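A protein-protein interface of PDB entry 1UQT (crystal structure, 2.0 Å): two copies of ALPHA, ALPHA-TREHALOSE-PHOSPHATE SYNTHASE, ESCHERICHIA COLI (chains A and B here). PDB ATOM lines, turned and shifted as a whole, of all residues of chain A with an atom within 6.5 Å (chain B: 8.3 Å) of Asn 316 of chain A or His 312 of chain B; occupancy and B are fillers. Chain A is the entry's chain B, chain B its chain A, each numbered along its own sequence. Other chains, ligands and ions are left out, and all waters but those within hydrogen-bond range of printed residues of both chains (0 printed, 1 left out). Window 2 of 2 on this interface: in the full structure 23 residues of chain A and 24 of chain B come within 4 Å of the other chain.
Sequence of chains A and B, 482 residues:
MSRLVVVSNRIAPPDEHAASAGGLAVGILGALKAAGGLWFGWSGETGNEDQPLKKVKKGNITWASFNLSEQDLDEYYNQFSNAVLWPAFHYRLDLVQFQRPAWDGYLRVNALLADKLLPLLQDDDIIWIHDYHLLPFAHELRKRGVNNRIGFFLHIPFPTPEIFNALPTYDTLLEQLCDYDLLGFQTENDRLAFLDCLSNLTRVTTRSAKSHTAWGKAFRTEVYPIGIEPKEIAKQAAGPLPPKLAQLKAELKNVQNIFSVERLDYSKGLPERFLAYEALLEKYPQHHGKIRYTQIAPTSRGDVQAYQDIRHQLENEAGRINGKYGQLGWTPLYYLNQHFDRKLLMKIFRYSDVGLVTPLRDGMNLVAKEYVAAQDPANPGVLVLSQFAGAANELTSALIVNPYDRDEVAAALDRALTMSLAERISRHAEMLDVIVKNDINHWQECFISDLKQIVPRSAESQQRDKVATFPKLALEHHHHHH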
ATOM      1  N   ARG A 311       3.718   7.549  33.712  1.00  0.00           N
ATOM      2  CA  ARG A 311       2.981   8.569  32.974  1.00  0.00           C
ATOM      3  C   ARG A 311       1.923   7.965  32.036  1.00  0.00           C
ATOM      4  O   ARG A 311       0.749   8.379  32.043  1.00  0.00           O
ATOM      5  CB  ARG A 311       3.939   9.436  32.169  1.00  0.00           C
ATOM      6  CG  ARG A 311       3.322  10.684  31.553  1.00  0.00           C
ATOM      7  CD  ARG A 311       4.382  11.587  30.867  1.00  0.00           C
ATOM      8  NE  ARG A 311       3.795  12.369  29.770  1.00  0.00           N
ATOM      9  CZ  ARG A 311       4.387  12.691  28.622  1.00  0.00           C
ATOM     10  NH1 ARG A 311       5.629  12.313  28.343  1.00  0.00           N
ATOM     11  NH2 ARG A 311       3.711  13.408  27.724  1.00  0.00           N
ATOM     12  N   HIS A 312       2.334   6.989  31.242  1.00  0.00           N
ATOM     13  CA  HIS A 312       1.430   6.345  30.280  1.00  0.00           C
ATOM     14  C   HIS A 312       0.296   5.577  30.980  1.00  0.00           C
ATOM     15  O   HIS A 312      -0.830   5.530  30.480  1.00  0.00           O
ATOM     16  CB  HIS A 312       2.214   5.412  29.336  1.00  0.00           C
ATOM     17  CG  HIS A 312       3.023   6.135  28.297  1.00  0.00           C
ATOM     18  ND1 HIS A 312       4.406   6.111  28.273  1.00  0.00           N
ATOM     19  CD2 HIS A 312       2.647   6.867  27.217  1.00  0.00           C
ATOM     20  CE1 HIS A 312       4.846   6.813  27.241  1.00  0.00           C
ATOM     21  NE2 HIS A 312       3.799   7.280  26.581  1.00  0.00           N
ATOM     22  N   GLN A 313       0.596   5.002  32.146  1.00  0.00           N
ATOM     23  CA  GLN A 313      -0.400   4.287  32.954  1.00  0.00           C
ATOM     24  C   GLN A 313      -1.441   5.262  33.507  1.00  0.00           C
ATOM     25  O   GLN A 313      -2.624   4.924  33.623  1.00  0.00           O
ATOM     26  CB  GLN A 313       0.251   3.515  34.125  1.00  0.00           C
ATOM     27  CG  GLN A 313       0.091   1.984  34.063  1.00  0.00           C
ATOM     28  CD  GLN A 313      -1.347   1.516  34.369  1.00  0.00           C
ATOM     29  OE1 GLN A 313      -2.082   1.113  33.463  1.00  0.00           O
ATOM     30  NE2 GLN A 313      -1.736   1.569  35.645  1.00  0.00           N
ATOM     31  N   LEU A 314      -1.006   6.471  33.835  1.00  0.00           N
ATOM     32  CA  LEU A 314      -1.893   7.470  34.393  1.00  0.00           C
ATOM     33  C   LEU A 314      -2.811   8.007  33.306  1.00  0.00           C
ATOM     34  O   LEU A 314      -3.971   8.226  33.555  1.00  0.00           O
ATOM     35  CB  LEU A 314      -1.090   8.627  35.014  1.00  0.00           C
ATOM     36  CG  LEU A 314      -1.009   8.761  36.525  1.00  0.00           C
ATOM     37  CD1 LEU A 314      -1.163   7.440  37.271  1.00  0.00           C
ATOM     38  CD2 LEU A 314       0.263   9.507  36.888  1.00  0.00           C
ATOM     39  N   GLU A 315      -2.266   8.226  32.111  1.00  0.00           N
ATOM     40  CA  GLU A 315      -3.054   8.653  30.969  1.00  0.00           C
ATOM     41  C   GLU A 315      -4.163   7.623  30.715  1.00  0.00           C
ATOM     42  O   GLU A 315      -5.332   7.963  30.613  1.00  0.00           O
ATOM     43  CB  GLU A 315      -2.160   8.773  29.755  1.00  0.00           C
ATOM     44  CG  GLU A 315      -1.176   9.940  29.836  1.00  0.00           C
ATOM     45  CD  GLU A 315      -0.095   9.885  28.762  1.00  0.00           C
ATOM     46  OE1 GLU A 315       0.047   8.865  28.072  1.00  0.00           O
ATOM     47  OE2 GLU A 315       0.635  10.866  28.623  1.00  0.00           O
ATOM     48  N   ASN A 316      -3.771   6.361  30.645  1.00  0.00           N
ATOM     49  CA  ASN A 316      -4.686   5.264  30.401  1.00  0.00           C
ATOM     50  C   ASN A 316      -5.766   5.206  31.471  1.00  0.00           C
ATOM     51  O   ASN A 316      -6.943   5.096  31.156  1.00  0.00           O
ATOM     52  CB  ASN A 316      -3.909   3.942  30.350  1.00  0.00           C
ATOM     53  CG  ASN A 316      -4.740   2.811  29.878  1.00  0.00           C
ATOM     54  OD1 ASN A 316      -5.222   2.006  30.713  1.00  0.00           O
ATOM     55  ND2 ASN A 316      -4.982   2.736  28.537  1.00  0.00           N
ATOM     56  N   GLU A 317      -5.358   5.317  32.731  1.00  0.00           N
ATOM     57  CA  GLU A 317      -6.275   5.221  33.858  1.00  0.00           C
ATOM     58  C   GLU A 317      -7.230   6.428  33.993  1.00  0.00           C
ATOM     59  O   GLU A 317      -8.389   6.281  34.386  1.00  0.00           O
ATOM     60  CB  GLU A 317      -5.491   4.968  35.149  1.00  0.00           C
ATOM     61  CG  GLU A 317      -4.923   3.563  35.215  1.00  0.00           C
ATOM     62  CD  GLU A 317      -6.020   2.504  35.399  1.00  0.00           C
ATOM     63  OE1 GLU A 317      -6.485   2.329  36.548  1.00  0.00           O
ATOM     64  OE2 GLU A 317      -6.429   1.877  34.385  1.00  0.00           O
ATOM     65  N   ALA A 318      -6.773   7.622  33.648  1.00  0.00           N
ATOM     66  CA  ALA A 318      -7.652   8.777  33.654  1.00  0.00           C
ATOM     67  C   ALA A 318      -8.742   8.543  32.632  1.00  0.00           C
ATOM     68  O   ALA A 318      -9.922   8.808  32.889  1.00  0.00           O
ATOM     69  CB  ALA A 318      -6.876  10.041  33.313  1.00  0.00           C
ATOM     70  N   GLY A 319      -8.342   8.064  31.460  1.00  0.00           N
ATOM     71  CA  GLY A 319      -9.259   7.813  30.360  1.00  0.00           C
ATOM     72  C   GLY A 319     -10.247   6.721  30.736  1.00  0.00           C
ATOM     73  O   GLY A 319     -11.453   6.864  30.528  1.00  0.00           O
ATOM     74  N   ARG A 320      -9.739   5.652  31.328  1.00  0.00           N
ATOM     75  CA  ARG A 320     -10.582   4.522  31.703  1.00  0.00           C
ATOM     76  C   ARG A 320     -11.620   4.915  32.760  1.00  0.00           C
ATOM     77  O   ARG A 320     -12.808   4.648  32.609  1.00  0.00           O
ATOM     78  CB  ARG A 320      -9.726   3.347  32.203  1.00  0.00           C
ATOM     79  CG  ARG A 320     -10.526   2.060  32.502  1.00  0.00           C
ATOM     80  CD  ARG A 320      -9.670   0.912  33.045  1.00  0.00           C
ATOM     81  NE  ARG A 320      -9.122   1.231  34.358  1.00  0.00           N
ATOM     82  CZ  ARG A 320      -9.807   1.284  35.503  1.00  0.00           C
ATOM     83  NH1 ARG A 320     -11.094   0.959  35.573  1.00  0.00           N
ATOM     84  NH2 ARG A 320      -9.178   1.624  36.619  1.00  0.00           N
ATOM     85  N   ILE A 321     -11.162   5.539  33.826  1.00  0.00           N
ATOM     86  CA  ILE A 321     -12.030   5.942  34.915  1.00  0.00           C
ATOM     87  C   ILE A 321     -13.081   6.984  34.517  1.00  0.00           C
ATOM     88  O   ILE A 321     -14.262   6.846  34.873  1.00  0.00           O
ATOM     89  CB  ILE A 321     -11.193   6.418  36.115  1.00  0.00           C
ATOM     90  CG1 ILE A 321     -10.405   5.235  36.664  1.00  0.00           C
ATOM     91  CG2 ILE A 321     -12.099   7.018  37.192  1.00  0.00           C
ATOM     92  CD1 ILE A 321      -9.317   5.610  37.627  1.00  0.00           C
ATOM     93  N   LEU B 264     -17.217   1.770  19.686  1.00  0.00           N
ATOM     94  CA  LEU B 264     -15.770   1.821  19.819  1.00  0.00           C
ATOM     95  C   LEU B 264     -15.165   0.756  18.907  1.00  0.00           C
ATOM     96  O   LEU B 264     -14.885  -0.365  19.322  1.00  0.00           O
ATOM     97  CB  LEU B 264     -15.342   1.632  21.285  1.00  0.00           C
ATOM     98  CG  LEU B 264     -14.096   2.446  21.659  1.00  0.00           C
ATOM     99  CD1 LEU B 264     -13.853   2.591  23.197  1.00  0.00           C
ATOM    100  CD2 LEU B 264     -12.909   1.852  20.975  1.00  0.00           C
ATOM    101  N   PRO B 271      -8.924   7.360  17.467  1.00  0.00           N
ATOM    102  CA  PRO B 271      -7.633   7.963  17.833  1.00  0.00           C
ATOM    103  C   PRO B 271      -7.194   9.057  16.861  1.00  0.00           C
ATOM    104  O   PRO B 271      -6.720  10.102  17.316  1.00  0.00           O
ATOM    105  CB  PRO B 271      -6.648   6.786  17.771  1.00  0.00           C
ATOM    106  CG  PRO B 271      -7.507   5.567  17.899  1.00  0.00           C
ATOM    107  CD  PRO B 271      -8.792   5.919  17.196  1.00  0.00           C
ATOM    108  N   GLY B 302     -16.014  -6.643  22.672  1.00  0.00           N
ATOM    109  CA  GLY B 302     -14.893  -6.530  23.581  1.00  0.00           C
ATOM    110  C   GLY B 302     -14.165  -7.835  23.871  1.00  0.00           C
ATOM    111  O   GLY B 302     -13.172  -7.823  24.577  1.00  0.00           O
ATOM    112  N   GLN B 305      -9.529  -9.306  20.467  1.00  0.00           N
ATOM    113  CA  GLN B 305      -8.288  -8.603  20.778  1.00  0.00           C
ATOM    114  C   GLN B 305      -8.120  -7.209  20.127  1.00  0.00           C
ATOM    115  O   GLN B 305      -7.780  -6.238  20.819  1.00  0.00           O
ATOM    116  CB  GLN B 305      -7.081  -9.497  20.495  1.00  0.00           C
ATOM    117  CG  GLN B 305      -5.763  -8.911  21.027  1.00  0.00           C
ATOM    118  CD  GLN B 305      -5.780  -8.692  22.543  1.00  0.00           C
ATOM    119  OE1 GLN B 305      -5.596  -7.555  23.026  1.00  0.00           O
ATOM    120  NE2 GLN B 305      -6.009  -9.763  23.290  1.00  0.00           N
ATOM    121  N   ALA B 306      -8.391  -7.086  18.828  1.00  0.00           N
ATOM    122  CA  ALA B 306      -8.210  -5.798  18.148  1.00  0.00           C
ATOM    123  C   ALA B 306      -9.124  -4.733  18.722  1.00  0.00           C
ATOM    124  O   ALA B 306      -8.742  -3.596  18.801  1.00  0.00           O
ATOM    125  CB  ALA B 306      -8.421  -5.929  16.688  1.00  0.00           C
ATOM    126  N   TYR B 307     -10.339  -5.105  19.142  1.00  0.00           N
ATOM    127  CA  TYR B 307     -11.218  -4.164  19.838  1.00  0.00           C
ATOM    128  C   TYR B 307     -10.697  -3.736  21.232  1.00  0.00           C
ATOM    129  O   TYR B 307     -10.799  -2.579  21.579  1.00  0.00           O
ATOM    130  CB  TYR B 307     -12.651  -4.706  19.921  1.00  0.00           C
ATOM    131  CG  TYR B 307     -13.358  -4.689  18.583  1.00  0.00           C
ATOM    132  CD1 TYR B 307     -13.179  -5.706  17.642  1.00  0.00           C
ATOM    133  CD2 TYR B 307     -14.166  -3.639  18.235  1.00  0.00           C
ATOM    134  CE1 TYR B 307     -13.831  -5.666  16.409  1.00  0.00           C
ATOM    135  CE2 TYR B 307     -14.812  -3.593  17.017  1.00  0.00           C
ATOM    136  CZ  TYR B 307     -14.649  -4.619  16.106  1.00  0.00           C
ATOM    137  OH  TYR B 307     -15.305  -4.537  14.890  1.00  0.00           O
ATOM    138  N   GLN B 308     -10.144  -4.639  22.026  1.00  0.00           N
ATOM    139  CA  GLN B 308      -9.532  -4.240  23.306  1.00  0.00           C
ATOM    140  C   GLN B 308      -8.355  -3.308  23.064  1.00  0.00           C
ATOM    141  O   GLN B 308      -8.149  -2.368  23.823  1.00  0.00           O
ATOM    142  CB  GLN B 308      -9.049  -5.432  24.128  1.00  0.00           C
ATOM    143  CG  GLN B 308     -10.165  -6.387  24.553  1.00  0.00           C
ATOM    144  CD  GLN B 308      -9.660  -7.701  25.133  1.00  0.00           C
ATOM    145  OE1 GLN B 308      -8.519  -7.798  25.578  1.00  0.00           O
ATOM    146  NE2 GLN B 308     -10.518  -8.706  25.143  1.00  0.00           N
ATOM    147  N   ASP B 309      -7.618  -3.532  21.976  1.00  0.00           N
ATOM    148  CA  ASP B 309      -6.445  -2.718  21.692  1.00  0.00           C
ATOM    149  C   ASP B 309      -6.848  -1.285  21.409  1.00  0.00           C
ATOM    150  O   ASP B 309      -6.232  -0.387  21.931  1.00  0.00           O
ATOM    151  CB  ASP B 309      -5.643  -3.263  20.490  1.00  0.00           C
ATOM    152  CG  ASP B 309      -4.906  -4.551  20.793  1.00  0.00           C
ATOM    153  OD1 ASP B 309      -4.795  -4.976  21.967  1.00  0.00           O
ATOM    154  OD2 ASP B 309      -4.373  -5.200  19.885  1.00  0.00           O
ATOM    155  N   ILE B 310      -7.861  -1.084  20.561  1.00  0.00           N
ATOM    156  CA  ILE B 310      -8.248   0.255  20.134  1.00  0.00           C
ATOM    157  C   ILE B 310      -8.858   1.015  21.310  1.00  0.00           C
ATOM    158  O   ILE B 310      -8.600   2.197  21.471  1.00  0.00           O
ATOM    159  CB  ILE B 310      -9.159   0.244  18.836  1.00  0.00           C
ATOM    160  CG1 ILE B 310      -9.364   1.650  18.313  1.00  0.00           C
ATOM    161  CG2 ILE B 310     -10.547  -0.385  19.071  1.00  0.00           C
ATOM    162  CD1 ILE B 310      -8.235   2.144  17.443  1.00  0.00           C
ATOM    163  N   ARG B 311      -9.615   0.309  22.157  1.00  0.00           N
ATOM    164  CA  ARG B 311     -10.127   0.884  23.401  1.00  0.00           C
ATOM    165  C   ARG B 311      -8.998   1.398  24.297  1.00  0.00           C
ATOM    166  O   ARG B 311      -9.066   2.542  24.766  1.00  0.00           O
ATOM    167  CB  ARG B 311     -10.982  -0.114  24.180  1.00  0.00           C
ATOM    168  CG  ARG B 311     -11.586   0.451  25.465  1.00  0.00           C
ATOM    169  CD  ARG B 311     -12.562  -0.509  26.183  1.00  0.00           C
ATOM    170  NE  ARG B 311     -12.652  -0.143  27.600  1.00  0.00           N
ATOM    171  CZ  ARG B 311     -13.401  -0.762  28.526  1.00  0.00           C
ATOM    172  NH1 ARG B 311     -14.166  -1.809  28.207  1.00  0.00           N
ATOM    173  NH2 ARG B 311     -13.367  -0.329  29.791  1.00  0.00           N
ATOM    174  N   HIS B 312      -7.979   0.579  24.537  1.00  0.00           N
ATOM    175  CA  HIS B 312      -6.858   1.020  25.376  1.00  0.00           C
ATOM    176  C   HIS B 312      -6.110   2.191  24.708  1.00  0.00           C
ATOM    177  O   HIS B 312      -5.684   3.123  25.386  1.00  0.00           O
ATOM    178  CB  HIS B 312      -5.863  -0.114  25.729  1.00  0.00           C
ATOM    179  CG  HIS B 312      -6.462  -1.235  26.541  1.00  0.00           C
ATOM    180  ND1 HIS B 312      -7.514  -1.055  27.425  1.00  0.00           N
ATOM    181  CD2 HIS B 312      -6.171  -2.562  26.573  1.00  0.00           C
ATOM    182  CE1 HIS B 312      -7.843  -2.218  27.961  1.00  0.00           C
ATOM    183  NE2 HIS B 312      -7.043  -3.149  27.465  1.00  0.00           N
ATOM    184  N   GLN B 313      -5.958   2.142  23.390  1.00  0.00           N
ATOM    185  CA  GLN B 313      -5.311   3.242  22.654  1.00  0.00           C
ATOM    186  C   GLN B 313      -6.109   4.537  22.844  1.00  0.00           C
ATOM    187  O   GLN B 313      -5.552   5.587  23.136  1.00  0.00           O
ATOM    188  CB  GLN B 313      -5.107   2.883  21.173  1.00  0.00           C
ATOM    189  CG  GLN B 313      -4.422   3.983  20.346  1.00  0.00           C
ATOM    190  CD  GLN B 313      -4.276   3.653  18.836  1.00  0.00           C
ATOM    191  OE1 GLN B 313      -3.586   4.384  18.121  1.00  0.00           O
ATOM    192  NE2 GLN B 313      -4.914   2.562  18.370  1.00  0.00           N
ATOM    193  N   LEU B 314      -7.434   4.443  22.754  1.00  0.00           N
ATOM    194  CA  LEU B 314      -8.294   5.617  22.859  1.00  0.00           C
ATOM    195  C   LEU B 314      -8.264   6.226  24.265  1.00  0.00           C
ATOM    196  O   LEU B 314      -8.191   7.464  24.417  1.00  0.00           O
ATOM    197  CB  LEU B 314      -9.717   5.253  22.463  1.00  0.00           C
ATOM    198  CG  LEU B 314     -10.613   6.438  22.095  1.00  0.00           C
ATOM    199  CD1 LEU B 314      -9.991   7.244  20.960  1.00  0.00           C
ATOM    200  CD2 LEU B 314     -12.006   5.930  21.696  1.00  0.00           C
ATOM    201  N   GLU B 315      -8.312   5.370  25.288  1.00  0.00           N
ATOM    202  CA  GLU B 315      -8.217   5.809  26.688  1.00  0.00           C
ATOM    203  C   GLU B 315      -6.921   6.564  26.909  1.00  0.00           C
ATOM    204  O   GLU B 315      -6.897   7.589  27.596  1.00  0.00           O
ATOM    205  CB  GLU B 315      -8.185   4.631  27.659  1.00  0.00           C
ATOM    206  CG  GLU B 315      -9.506   3.904  27.860  1.00  0.00           C
ATOM    207  CD  GLU B 315      -9.310   2.535  28.522  1.00  0.00           C
ATOM    208  OE1 GLU B 315      -8.147   2.073  28.732  1.00  0.00           O
ATOM    209  OE2 GLU B 315     -10.315   1.902  28.839  1.00  0.00           O
ATOM    210  N   ASN B 316      -5.834   6.035  26.352  1.00  0.00           N
ATOM    211  CA  ASN B 316      -4.551   6.680  26.538  1.00  0.00           C
ATOM    212  C   ASN B 316      -4.619   8.076  25.978  1.00  0.00           C
ATOM    213  O   ASN B 316      -4.129   9.002  26.590  1.00  0.00           O
ATOM    214  CB  ASN B 316      -3.403   5.947  25.873  1.00  0.00           C
ATOM    215  CG  ASN B 316      -2.049   6.619  26.167  1.00  0.00           C
ATOM    216  OD1 ASN B 316      -1.563   7.459  25.371  1.00  0.00           O
ATOM    217  ND2 ASN B 316      -1.466   6.294  27.330  1.00  0.00           N
ATOM    218  N   GLU B 317      -5.250   8.233  24.825  1.00  0.00           N
ATOM    219  CA  GLU B 317      -5.234   9.511  24.136  1.00  0.00           C
ATOM    220  C   GLU B 317      -6.116  10.543  24.825  1.00  0.00           C
ATOM    221  O   GLU B 317      -5.754  11.714  24.847  1.00  0.00           O
ATOM    222  CB  GLU B 317      -5.595   9.341  22.675  1.00  0.00           C
ATOM    223  CG  GLU B 317      -4.483   8.676  21.867  1.00  0.00           C
ATOM    224  CD  GLU B 317      -3.242   9.559  21.765  1.00  0.00           C
ATOM    225  OE1 GLU B 317      -3.219  10.456  20.933  1.00  0.00           O
ATOM    226  OE2 GLU B 317      -2.310   9.386  22.567  1.00  0.00           O
ATOM    227  N   ALA B 318      -7.235  10.106  25.415  1.00  0.00           N
ATOM    228  CA  ALA B 318      -8.079  10.982  26.220  1.00  0.00           C
ATOM    229  C   ALA B 318      -7.302  11.531  27.374  1.00  0.00           C
ATOM    230  O   ALA B 318      -7.363  12.710  27.649  1.00  0.00           O
ATOM    231  CB  ALA B 318      -9.330  10.253  26.769  1.00  0.00           C
ATOM    232  N   GLY B 319      -6.573  10.667  28.062  1.00  0.00           N
ATOM    233  CA  GLY B 319      -5.828  11.068  29.225  1.00  0.00           C
ATOM    234  C   GLY B 319      -4.682  11.982  28.842  1.00  0.00           C
ATOM    235  O   GLY B 319      -4.389  12.927  29.560  1.00  0.00           O
ATOM    236  N   ARG B 320      -4.021  11.680  27.726  1.00  0.00           N
ATOM    237  CA  ARG B 320      -2.883  12.455  27.285  1.00  0.00           C
ATOM    238  C   ARG B 320      -3.322  13.854  26.914  1.00  0.00           C
ATOM    239  O   ARG B 320      -2.755  14.841  27.393  1.00  0.00           O
ATOM    240  CB  ARG B 320      -2.204  11.800  26.090  1.00  0.00           C
ATOM    241  CG  ARG B 320      -0.842  12.416  25.787  1.00  0.00           C
ATOM    242  CD  ARG B 320      -0.144  11.854  24.560  1.00  0.00           C
ATOM    243  NE  ARG B 320      -0.956  11.974  23.358  1.00  0.00           N
ATOM    244  CZ  ARG B 320      -1.127  13.068  22.618  1.00  0.00           C
ATOM    245  NH1 ARG B 320      -0.557  14.207  22.926  1.00  0.00           N
ATOM    246  NH2 ARG B 320      -1.905  13.012  21.543  1.00  0.00           N
ATOM    247  N   TYR B 335     -14.726  11.836  27.280  1.00  0.00           N
ATOM    248  CA  TYR B 335     -14.823  10.524  26.681  1.00  0.00           C
ATOM    249  C   TYR B 335     -15.679   9.643  27.557  1.00  0.00           C
ATOM    250  O   TYR B 335     -15.401   9.483  28.710  1.00  0.00           O
ATOM    251  CB  TYR B 335     -13.423   9.938  26.528  1.00  0.00           C
ATOM    252  CG  TYR B 335     -13.345   8.457  26.348  1.00  0.00           C
ATOM    253  CD1 TYR B 335     -13.850   7.820  25.205  1.00  0.00           C
ATOM    254  CD2 TYR B 335     -12.757   7.671  27.326  1.00  0.00           C
ATOM    255  CE1 TYR B 335     -13.731   6.438  25.058  1.00  0.00           C
ATOM    256  CE2 TYR B 335     -12.651   6.310  27.185  1.00  0.00           C
ATOM    257  CZ  TYR B 335     -13.146   5.683  26.069  1.00  0.00           C
ATOM    258  OH  TYR B 335     -13.020   4.296  26.010  1.00  0.00           O
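The side-chain carboxylate (OE2) of Glu 315 of chain B lies within salt-bridge range of the guanidinium group (NE) of Arg 311 of chain B (3.3 Å). OE1 of Glu 315 of chain B lies within hydrogen-bond range of ND1 of His 312 of chain B, 3.4 Å away. OD1 of Asn 316 of chain B sits close to OE2 of Glu 317 of chain B (3.5 Å). The side-chain carboxylate (OE1) of Glu 317 of chain B is in salt-bridge range of the guanidinium group (NH2) of Arg 320 of chain B (2.9 Å). The side-chain carboxylate (OE2) of Glu 315 of chain A is in salt-bridge range of the guanidinium group (NE) of Arg 311 of chain A (3.7 Å). OE2 of Glu 317 of chain A lies within salt-bridge range of NE of Arg 320 of chain A (2.8 Å).
Asn 316 of chain A touches two residues of chain B. Ala 318 of chain A touches none of the printed residues of chain B. Of the printed residues of chain B, Arg 320 of chain A touches Glu 315 (3.7 Å). Of chain A, only Asn 316 comes within 4 Å of His 312 of chain B. Gln 313 of chain B touches none of the printed residues of chain A. Printed residues of chain A within 4 Å of Asn 316 of chain B: His 312 (3.3 Å) and Glu 315 (3.1 Å). The nearest residue of chain B that does not touch Asn 316 of chain A is Asn 316 of chain B (4.04 Å). The nearest residue of chain A that does not touch His 312 of chain B is Arg 320 of chain A (6.2 Å).
The side-chain amide nitrogen (ND2) of Asn 316 of chain A lies within hydrogen-bond range of the backbone carbonyl oxygen (O) of His 312 of chain B, 3.3 Å away. The side-chain amide nitrogen (ND2) of Asn 316 of chain A is in hydrogen-bond range of the side-chain carboxylate (OE1) of Glu 315 of chain B (3.2 Å). ND2 of Asn 316 of chain B sits at hydrogen-bond distance from O of His 312 of chain A, at 3.3 Å. OE1 of Glu 315 of chain A sits at hydrogen-bond distance from ND2 of Asn 316 of chain B, 3.1 Å away. The backbone carbonyl oxygen of Glu 315 of chain A lies close to the backbone carbonyl oxygen of Glu 315 of chain B (3.4 Å).
Of the 11 printed residues of chain A, 5 touch a printed residue of chain B. Along chain A the printed residues that touch a printed residue of chain B span positions 312 to 320. Printed residues of chain B that touch a printed residue of chain A: His 312, Glu 315, Asn 316, Gly 319, Arg 320 and Tyr 335. Hydrophobic or aromatic side chains of chain B that line the printed part of chain A: Tyr 335.
His 312 of chain A touches Asn 316 of chain B, and with the chains exchanged Asn 316 of chain A touches His 312 of chain B. Glu 315 of chain B touches its own counterpart, Glu 315 of chain A. Glu 315 of chain A touches Asn 316 of chain B, and with the chains exchanged Asn 316 of chain A touches Glu 315 of chain B. Glu 315 of chain A touches Gly 319 of chain B, and with the chains exchanged Gly 319 of chain A touches Glu 315 of chain B. Of the 10 pairs that touch across the chains among the printed residues, 9 have their exchanged pair printed and touching as well.
Among the printed residues, pairs that only touch across the chains: Glu 315 of chain A with Gly 319 of chain B (3.4 Å), Gly 319 of chain A with Tyr 335 of chain B (3.6 Å), Glu 315 of chain A with Arg 320 of chain B (3.6 Å), Gly 319 of chain A with Glu 315 of chain B (3.6 Å) and Arg 320 of chain A with Glu 315 of chain B (3.7 Å).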
